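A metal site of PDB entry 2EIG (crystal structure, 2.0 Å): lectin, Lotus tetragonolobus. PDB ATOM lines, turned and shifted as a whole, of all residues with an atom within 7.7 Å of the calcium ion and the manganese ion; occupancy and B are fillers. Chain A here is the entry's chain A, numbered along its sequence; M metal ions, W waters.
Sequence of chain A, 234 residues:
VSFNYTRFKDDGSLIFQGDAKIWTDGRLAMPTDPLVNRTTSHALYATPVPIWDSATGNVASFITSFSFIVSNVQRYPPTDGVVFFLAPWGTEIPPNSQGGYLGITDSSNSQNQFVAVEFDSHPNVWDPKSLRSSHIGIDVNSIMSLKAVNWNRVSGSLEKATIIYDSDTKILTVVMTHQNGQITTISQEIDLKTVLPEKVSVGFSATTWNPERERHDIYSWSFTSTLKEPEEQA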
ATOM      1  N   THR A  79     -14.367 -24.419 -12.720  1.00  0.00           N
ATOM      2  CA  THR A  79     -15.308 -23.978 -11.698  1.00  0.00           C
ATOM      3  C   THR A  79     -16.148 -25.175 -11.301  1.00  0.00           C
ATOM      4  O   THR A  79     -16.168 -26.141 -12.026  1.00  0.00           O
ATOM      5  CB  THR A  79     -16.234 -22.791 -12.115  1.00  0.00           C
ATOM      6  OG1 THR A  79     -17.448 -23.219 -12.720  1.00  0.00           O
ATOM      7  CG2 THR A  79     -15.531 -21.827 -12.990  1.00  0.00           C
ATOM      8  N   ASP A  80     -16.783 -25.140 -10.127  1.00  0.00           N
ATOM      9  CA  ASP A  80     -16.645 -24.012  -9.191  1.00  0.00           C
ATOM     10  C   ASP A  80     -15.988 -24.430  -7.907  1.00  0.00           C
ATOM     11  O   ASP A  80     -15.384 -23.634  -7.229  1.00  0.00           O
ATOM     12  CB  ASP A  80     -18.035 -23.423  -8.896  1.00  0.00           C
ATOM     13  CG  ASP A  80     -18.361 -22.251  -9.793  1.00  0.00           C
ATOM     14  OD1 ASP A  80     -17.912 -21.158  -9.432  1.00  0.00           O
ATOM     15  OD2 ASP A  80     -19.053 -22.450 -10.839  1.00  0.00           O
ATOM     16  N   GLY A  81     -16.162 -25.670  -7.511  1.00  0.00           N
ATOM     17  CA  GLY A  81     -15.432 -26.164  -6.379  1.00  0.00           C
ATOM     18  C   GLY A  81     -16.204 -27.281  -5.795  1.00  0.00           C
ATOM     19  O   GLY A  81     -17.271 -27.604  -6.278  1.00  0.00           O
ATOM     20  N   GLY A  99     -23.314 -22.627  -9.451  1.00  0.00           N
ATOM     21  CA  GLY A  99     -22.038 -21.973  -9.742  1.00  0.00           C
ATOM     22  C   GLY A  99     -21.226 -21.685  -8.476  1.00  0.00           C
ATOM     23  O   GLY A  99     -20.949 -22.588  -7.653  1.00  0.00           O
ATOM     24  N   GLY A 100     -20.856 -20.421  -8.331  1.00  0.00           N
ATOM     25  CA  GLY A 100     -19.963 -20.007  -7.270  1.00  0.00           C
ATOM     26  C   GLY A 100     -20.557 -20.079  -5.862  1.00  0.00           C
ATOM     27  O   GLY A 100     -19.816 -19.932  -4.880  1.00  0.00           O
ATOM     28  N   TYR A 101     -21.880 -20.271  -5.798  1.00  0.00           N
ATOM     29  CA  TYR A 101     -22.602 -20.484  -4.513  1.00  0.00           C
ATOM     30  C   TYR A 101     -22.488 -21.922  -4.000  1.00  0.00           C
ATOM     31  O   TYR A 101     -22.965 -22.233  -2.917  1.00  0.00           O
ATOM     32  CB  TYR A 101     -24.047 -20.050  -4.611  1.00  0.00           C
ATOM     33  CG  TYR A 101     -24.148 -18.574  -4.877  1.00  0.00           C
ATOM     34  CD1 TYR A 101     -23.825 -17.656  -3.842  1.00  0.00           C
ATOM     35  CD2 TYR A 101     -24.492 -18.088  -6.152  1.00  0.00           C
ATOM     36  CE1 TYR A 101     -23.847 -16.283  -4.074  1.00  0.00           C
ATOM     37  CE2 TYR A 101     -24.523 -16.692  -6.398  1.00  0.00           C
ATOM     38  CZ  TYR A 101     -24.207 -15.802  -5.346  1.00  0.00           C
ATOM     39  OH  TYR A 101     -24.227 -14.412  -5.507  1.00  0.00           O
ATOM     40  N   LEU A 102     -21.814 -22.778  -4.788  1.00  0.00           N
ATOM     41  CA  LEU A 102     -21.314 -24.081  -4.345  1.00  0.00           C
ATOM     42  C   LEU A 102     -22.360 -25.100  -3.892  1.00  0.00           C
ATOM     43  O   LEU A 102     -22.009 -26.120  -3.321  1.00  0.00           O
ATOM     44  CB  LEU A 102     -20.149 -23.936  -3.319  1.00  0.00           C
ATOM     45  CG  LEU A 102     -18.869 -23.322  -3.946  1.00  0.00           C
ATOM     46  CD1 LEU A 102     -17.837 -22.899  -2.916  1.00  0.00           C
ATOM     47  CD2 LEU A 102     -18.167 -24.242  -5.009  1.00  0.00           C
ATOM     48  N   GLU A 118     -14.371 -25.294   1.810  1.00  0.00           N
ATOM     49  CA  GLU A 118     -14.523 -25.231   0.376  1.00  0.00           C
ATOM     50  C   GLU A 118     -13.175 -25.319  -0.291  1.00  0.00           C
ATOM     51  O   GLU A 118     -12.162 -24.854   0.202  1.00  0.00           O
ATOM     52  CB  GLU A 118     -15.247 -23.940  -0.093  1.00  0.00           C
ATOM     53  CG  GLU A 118     -14.417 -22.697   0.227  1.00  0.00           C
ATOM     54  CD  GLU A 118     -14.950 -21.432  -0.403  1.00  0.00           C
ATOM     55  OE1 GLU A 118     -16.151 -21.147  -0.328  1.00  0.00           O
ATOM     56  OE2 GLU A 118     -14.121 -20.716  -0.958  1.00  0.00           O
ATOM     57  N   PHE A 119     -13.205 -25.905  -1.467  1.00  0.00           N
ATOM     58  CA  PHE A 119     -12.030 -26.050  -2.275  1.00  0.00           C
ATOM     59  C   PHE A 119     -12.596 -25.373  -3.521  1.00  0.00           C
ATOM     60  O   PHE A 119     -13.336 -25.950  -4.292  1.00  0.00           O
ATOM     61  CB  PHE A 119     -11.709 -27.528  -2.506  1.00  0.00           C
ATOM     62  CG  PHE A 119     -11.255 -28.257  -1.260  1.00  0.00           C
ATOM     63  CD1 PHE A 119     -12.173 -28.905  -0.449  1.00  0.00           C
ATOM     64  CD2 PHE A 119      -9.899 -28.255  -0.885  1.00  0.00           C
ATOM     65  CE1 PHE A 119     -11.779 -29.583   0.704  1.00  0.00           C
ATOM     66  CE2 PHE A 119      -9.496 -28.926   0.259  1.00  0.00           C
ATOM     67  CZ  PHE A 119     -10.430 -29.601   1.067  1.00  0.00           C
ATOM     68  N   ASP A 120     -12.246 -24.119  -3.674  1.00  0.00           N
ATOM     69  CA  ASP A 120     -12.905 -23.251  -4.589  1.00  0.00           C
ATOM     70  C   ASP A 120     -11.906 -23.009  -5.728  1.00  0.00           C
ATOM     71  O   ASP A 120     -10.814 -22.518  -5.500  1.00  0.00           O
ATOM     72  CB  ASP A 120     -13.242 -21.941  -3.847  1.00  0.00           C
ATOM     73  CG  ASP A 120     -14.050 -20.970  -4.669  1.00  0.00           C
ATOM     74  OD1 ASP A 120     -14.713 -20.094  -4.092  1.00  0.00           O
ATOM     75  OD2 ASP A 120     -14.028 -21.002  -5.906  1.00  0.00           O
ATOM     76  N   SER A 121     -12.308 -23.378  -6.937  1.00  0.00           N
ATOM     77  CA  SER A 121     -11.397 -23.374  -8.094  1.00  0.00           C
ATOM     78  C   SER A 121     -11.562 -22.108  -8.943  1.00  0.00           C
ATOM     79  O   SER A 121     -10.983 -22.000  -9.985  1.00  0.00           O
ATOM     80  CB  SER A 121     -11.706 -24.583  -8.962  1.00  0.00           C
ATOM     81  OG  SER A 121     -13.086 -24.637  -9.288  1.00  0.00           O
ATOM     82  N   HIS A 122     -12.469 -21.221  -8.562  1.00  0.00           N
ATOM     83  CA  HIS A 122     -12.827 -20.078  -9.410  1.00  0.00           C
ATOM     84  C   HIS A 122     -13.072 -18.799  -8.595  1.00  0.00           C
ATOM     85  O   HIS A 122     -13.975 -18.781  -7.763  1.00  0.00           O
ATOM     86  CB  HIS A 122     -14.094 -20.392 -10.196  1.00  0.00           C
ATOM     87  CG  HIS A 122     -14.581 -19.241 -11.023  1.00  0.00           C
ATOM     88  ND1 HIS A 122     -14.018 -18.903 -12.228  1.00  0.00           N
ATOM     89  CD2 HIS A 122     -15.604 -18.370 -10.829  1.00  0.00           C
ATOM     90  CE1 HIS A 122     -14.652 -17.860 -12.739  1.00  0.00           C
ATOM     91  NE2 HIS A 122     -15.601 -17.505 -11.898  1.00  0.00           N
ATOM     92  N   PRO A 123     -12.271 -17.734  -8.845  1.00  0.00           N
ATOM     93  CA  PRO A 123     -12.444 -16.445  -8.158  1.00  0.00           C
ATOM     94  C   PRO A 123     -13.725 -15.742  -8.582  1.00  0.00           C
ATOM     95  O   PRO A 123     -13.864 -15.292  -9.718  1.00  0.00           O
ATOM     96  CB  PRO A 123     -11.220 -15.630  -8.568  1.00  0.00           C
ATOM     97  CG  PRO A 123     -10.302 -16.613  -9.177  1.00  0.00           C
ATOM     98  CD  PRO A 123     -11.154 -17.676  -9.787  1.00  0.00           C
ATOM     99  N   ASN A 124     -14.664 -15.717  -7.665  1.00  0.00           N
ATOM    100  CA  ASN A 124     -15.874 -14.960  -7.830  1.00  0.00           C
ATOM    101  C   ASN A 124     -15.569 -13.584  -7.213  1.00  0.00           C
ATOM    102  O   ASN A 124     -14.516 -13.371  -6.608  1.00  0.00           O
ATOM    103  CB  ASN A 124     -17.012 -15.656  -7.095  1.00  0.00           C
ATOM    104  CG  ASN A 124     -17.494 -16.937  -7.787  1.00  0.00           C
ATOM    105  OD1 ASN A 124     -17.147 -18.051  -7.355  1.00  0.00           O
ATOM    106  ND2 ASN A 124     -18.272 -16.789  -8.854  1.00  0.00           N
ATOM    107  N   VAL A 125     -16.515 -12.667  -7.329  1.00  0.00           N
ATOM    108  CA  VAL A 125     -16.373 -11.315  -6.805  1.00  0.00           C
ATOM    109  C   VAL A 125     -16.116 -11.244  -5.286  1.00  0.00           C
ATOM    110  O   VAL A 125     -15.472 -10.301  -4.823  1.00  0.00           O
ATOM    111  CB  VAL A 125     -17.619 -10.424  -7.221  1.00  0.00           C
ATOM    112  CG1 VAL A 125     -17.833 -10.476  -8.740  1.00  0.00           C
ATOM    113  CG2 VAL A 125     -18.818 -10.945  -6.590  1.00  0.00           C
ATOM    114  N   TRP A 126     -16.590 -12.274  -4.534  1.00  0.00           N
ATOM    115  CA  TRP A 126     -16.567 -12.277  -3.081  1.00  0.00           C
ATOM    116  C   TRP A 126     -15.411 -13.102  -2.559  1.00  0.00           C
ATOM    117  O   TRP A 126     -15.179 -13.207  -1.345  1.00  0.00           O
ATOM    118  CB  TRP A 126     -17.888 -12.869  -2.577  1.00  0.00           C
ATOM    119  CG  TRP A 126     -18.172 -14.263  -3.212  1.00  0.00           C
ATOM    120  CD1 TRP A 126     -17.573 -15.440  -2.913  1.00  0.00           C
ATOM    121  CD2 TRP A 126     -19.106 -14.562  -4.285  1.00  0.00           C
ATOM    122  NE1 TRP A 126     -18.093 -16.456  -3.681  1.00  0.00           N
ATOM    123  CE2 TRP A 126     -19.041 -15.947  -4.519  1.00  0.00           C
ATOM    124  CE3 TRP A 126     -19.991 -13.782  -5.043  1.00  0.00           C
ATOM    125  CZ2 TRP A 126     -19.827 -16.580  -5.481  1.00  0.00           C
ATOM    126  CZ3 TRP A 126     -20.764 -14.398  -6.001  1.00  0.00           C
ATOM    127  CH2 TRP A 126     -20.659 -15.804  -6.227  1.00  0.00           C
ATOM    128  N   ASP A 127     -14.706 -13.730  -3.491  1.00  0.00           N
ATOM    129  CA  ASP A 127     -13.564 -14.551  -3.204  1.00  0.00           C
ATOM    130  C   ASP A 127     -12.338 -13.726  -2.905  1.00  0.00           C
ATOM    131  O   ASP A 127     -12.277 -12.567  -3.292  1.00  0.00           O
ATOM    132  CB  ASP A 127     -13.314 -15.499  -4.384  1.00  0.00           C
ATOM    133  CG  ASP A 127     -14.209 -16.679  -4.330  1.00  0.00           C
ATOM    134  OD1 ASP A 127     -14.538 -17.048  -3.190  1.00  0.00           O
ATOM    135  OD2 ASP A 127     -14.634 -17.174  -5.393  1.00  0.00           O
ATOM    136  N   PRO A 128     -11.374 -14.335  -2.202  1.00  0.00           N
ATOM    137  CA  PRO A 128     -10.220 -13.579  -1.744  1.00  0.00           C
ATOM    138  C   PRO A 128      -9.592 -12.796  -2.907  1.00  0.00           C
ATOM    139  O   PRO A 128      -8.946 -13.384  -3.817  1.00  0.00           O
ATOM    140  CB  PRO A 128      -9.297 -14.645  -1.152  1.00  0.00           C
ATOM    141  CG  PRO A 128     -10.176 -15.791  -0.772  1.00  0.00           C
ATOM    142  CD  PRO A 128     -11.361 -15.737  -1.731  1.00  0.00           C
ATOM    143  N   SER A 133      -6.407 -17.159  -6.829  1.00  0.00           N
ATOM    144  CA  SER A 133      -7.293 -17.792  -7.760  1.00  0.00           C
ATOM    145  C   SER A 133      -8.015 -18.900  -6.919  1.00  0.00           C
ATOM    146  O   SER A 133      -8.911 -18.604  -6.100  1.00  0.00           O
ATOM    147  CB  SER A 133      -6.449 -18.342  -8.905  1.00  0.00           C
ATOM    148  OG  SER A 133      -7.243 -19.005  -9.864  1.00  0.00           O
ATOM    149  N   SER A 134      -7.583 -20.143  -7.078  1.00  0.00           N
ATOM    150  CA  SER A 134      -8.109 -21.236  -6.256  1.00  0.00           C
ATOM    151  C   SER A 134      -7.686 -21.041  -4.821  1.00  0.00           C
ATOM    152  O   SER A 134      -6.599 -20.552  -4.521  1.00  0.00           O
ATOM    153  CB  SER A 134      -7.628 -22.608  -6.769  1.00  0.00           C
ATOM    154  OG  SER A 134      -8.108 -22.815  -8.065  1.00  0.00           O
ATOM    155  N   HIS A 135      -8.579 -21.397  -3.925  1.00  0.00           N
ATOM    156  CA  HIS A 135      -8.329 -21.209  -2.532  1.00  0.00           C
ATOM    157  C   HIS A 135      -9.082 -22.259  -1.718  1.00  0.00           C
ATOM    158  O   HIS A 135     -10.075 -22.851  -2.173  1.00  0.00           O
ATOM    159  CB  HIS A 135      -8.743 -19.804  -2.133  1.00  0.00           C
ATOM    160  CG  HIS A 135     -10.129 -19.436  -2.547  1.00  0.00           C
ATOM    161  ND1 HIS A 135     -10.460 -19.057  -3.820  1.00  0.00           N
ATOM    162  CD2 HIS A 135     -11.264 -19.384  -1.835  1.00  0.00           C
ATOM    163  CE1 HIS A 135     -11.752 -18.779  -3.881  1.00  0.00           C
ATOM    164  NE2 HIS A 135     -12.261 -18.965  -2.668  1.00  0.00           N
ATOM    165  N   ILE A 136      -8.572 -22.518  -0.530  1.00  0.00           N
ATOM    166  CA  ILE A 136      -9.245 -23.403   0.394  1.00  0.00           C
ATOM    167  C   ILE A 136      -9.823 -22.427   1.427  1.00  0.00           C
ATOM    168  O   ILE A 136      -9.068 -21.603   1.963  1.00  0.00           O
ATOM    169  CB  ILE A 136      -8.253 -24.446   1.002  1.00  0.00           C
ATOM    170  CG1 ILE A 136      -7.765 -25.430  -0.066  1.00  0.00           C
ATOM    171  CG2 ILE A 136      -8.934 -25.256   2.161  1.00  0.00           C
ATOM    172  CD1 ILE A 136      -6.203 -25.790   0.068  1.00  0.00           C
ATOM    173  N   GLY A 137     -11.126 -22.494   1.669  1.00  0.00           N
ATOM    174  CA  GLY A 137     -11.745 -21.596   2.633  1.00  0.00           C
ATOM    175  C   GLY A 137     -12.570 -22.269   3.703  1.00  0.00           C
ATOM    176  O   GLY A 137     -13.106 -23.347   3.478  1.00  0.00           O
ATOM    177  N   ASP A 139     -16.049 -21.542   5.562  1.00  0.00           N
ATOM    178  CA  ASP A 139     -17.276 -20.803   5.364  1.00  0.00           C
ATOM    179  C   ASP A 139     -18.270 -21.099   6.497  1.00  0.00           C
ATOM    180  O   ASP A 139     -18.576 -22.279   6.797  1.00  0.00           O
ATOM    181  CB  ASP A 139     -17.979 -21.239   4.079  1.00  0.00           C
ATOM    182  CG  ASP A 139     -17.107 -21.135   2.867  1.00  0.00           C
ATOM    183  OD1 ASP A 139     -17.539 -21.716   1.872  1.00  0.00           O
ATOM    184  OD2 ASP A 139     -16.020 -20.500   2.924  1.00  0.00           O
ATOM    185  N   ILE A 143     -20.950 -17.397   1.729  1.00  0.00           N
ATOM    186  CA  ILE A 143     -20.051 -17.813   0.634  1.00  0.00           C
ATOM    187  C   ILE A 143     -18.721 -17.078   0.719  1.00  0.00           C
ATOM    188  O   ILE A 143     -17.719 -17.488   0.130  1.00  0.00           O
ATOM    189  CB  ILE A 143     -20.713 -17.615  -0.791  1.00  0.00           C
ATOM    190  CG1 ILE A 143     -20.180 -18.619  -1.823  1.00  0.00           C
ATOM    191  CG2 ILE A 143     -20.567 -16.115  -1.293  1.00  0.00           C
ATOM    192  CD1 ILE A 143     -20.196 -20.151  -1.385  1.00  0.00           C
ATOM    193  N   MET A 144     -18.699 -15.964   1.466  1.00  0.00           N
ATOM    194  CA  MET A 144     -17.411 -15.328   1.712  1.00  0.00           C
ATOM    195  C   MET A 144     -16.733 -15.961   2.873  1.00  0.00           C
ATOM    196  O   MET A 144     -17.215 -15.869   4.012  1.00  0.00           O
ATOM    197  CB  MET A 144     -17.543 -13.819   1.953  1.00  0.00           C
ATOM    198  CG  MET A 144     -17.925 -13.106   0.761  1.00  0.00           C
ATOM    199  SD  MET A 144     -19.274 -11.996   1.186  1.00  0.00           S
ATOM    200  CE  MET A 144     -20.615 -13.191   1.287  1.00  0.00           C
ATOM    201  N   SER A 145     -15.585 -16.551   2.612  1.00  0.00           N
ATOM    202  CA  SER A 145     -14.893 -17.327   3.611  1.00  0.00           C
ATOM    203  C   SER A 145     -14.459 -16.460   4.787  1.00  0.00           C
ATOM    204  O   SER A 145     -14.087 -15.298   4.613  1.00  0.00           O
ATOM    205  CB  SER A 145     -13.692 -17.997   2.971  1.00  0.00           C
ATOM    206  OG  SER A 145     -14.195 -18.860   1.971  1.00  0.00           O
ATOM    207  N   ALA A 148      -9.316 -17.980   4.505  1.00  0.00           N
ATOM    208  CA  ALA A 148      -9.006 -18.747   3.314  1.00  0.00           C
ATOM    209  C   ALA A 148      -7.519 -18.733   3.065  1.00  0.00           C
ATOM    210  O   ALA A 148      -6.778 -17.830   3.507  1.00  0.00           O
ATOM    211  CB  ALA A 148      -9.798 -18.213   2.091  1.00  0.00           C
HETATM  212 CA    CA M   1     -15.681 -19.187  -6.155  1.00  0.00          CA
HETATM  213 MN    MN M   2     -14.416 -18.948  -2.215  1.00  0.00          MN
HETATM  214  O   HOH W   1     -13.984 -17.760  -0.370  1.00  0.00           O
HETATM  215  O   HOH W   2     -16.547 -19.013  -1.784  1.00  0.00           O
HETATM  216  O   HOH W   3     -17.423 -19.227  -4.663  1.00  0.00           O
HETATM  217  O   HOH W   4     -16.642 -20.960  -7.350  1.00  0.00           O
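The side-chain hydroxyl (OG) of Ser 145 sits close to the side-chain carboxylate (OE2) of Glu 118, 3.5 Å away.
The side-chain carboxylate of Glu 118 lies close to the side-chain carboxylate of Asp 139.
The backbone carbonyl oxygen (O) of Gly 137 lies within hydrogen-bond range of the backbone NH (N) of Glu 118, 2.9 Å away.
O of Ser 133 is in hydrogen-bond range of ND1 of His 135, at 2.8 Å.
Within 4 Å of the calcium ion: Asp 120, His 122, Asn 124 and Asp 127.
The nearest printed residue that does not touch the calcium ion is Gly 100 (4.4 Å).
Four residues have an atom within 4 Å of the manganese ion: Glu 118, Asp 120, Asp 127 and His 135.
Along chain A the residues within 4 Å of the manganese ion span positions 118 to 135.
The side-chain amide oxygen (OD1) of Asn 124 is bound to the calcium ion.
Water W3 is bound to the calcium ion, at 2.3 Å.
Water W4 is bound to the calcium ion (2.3 Å).
O of His 122 is bound to the calcium ion.
The side-chain carboxylate (OD2) of Asp 127 binds the calcium ion, at 2.4 Å.
OD1 of Asp 120 binds the calcium ion (2.5 Å).
The side-chain carboxylate (OD2) of Asp 120 is bound to the calcium ion, at 2.5 Å.
The manganese ion is bound by OD1 of Asp 127, water W2, OE2 of Glu 118, NE2 of His 135, OD1 of Asp 120 and water W1.
Water W3 bridges O of Gly 100 (2.5 Å) and NE1 of Trp 126 (3.0 Å).
Water W2 bridges the side-chain carboxylate of Glu 118 (2.6 Å) and the backbone carbonyl oxygen of Ile 143 (2.7 Å).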
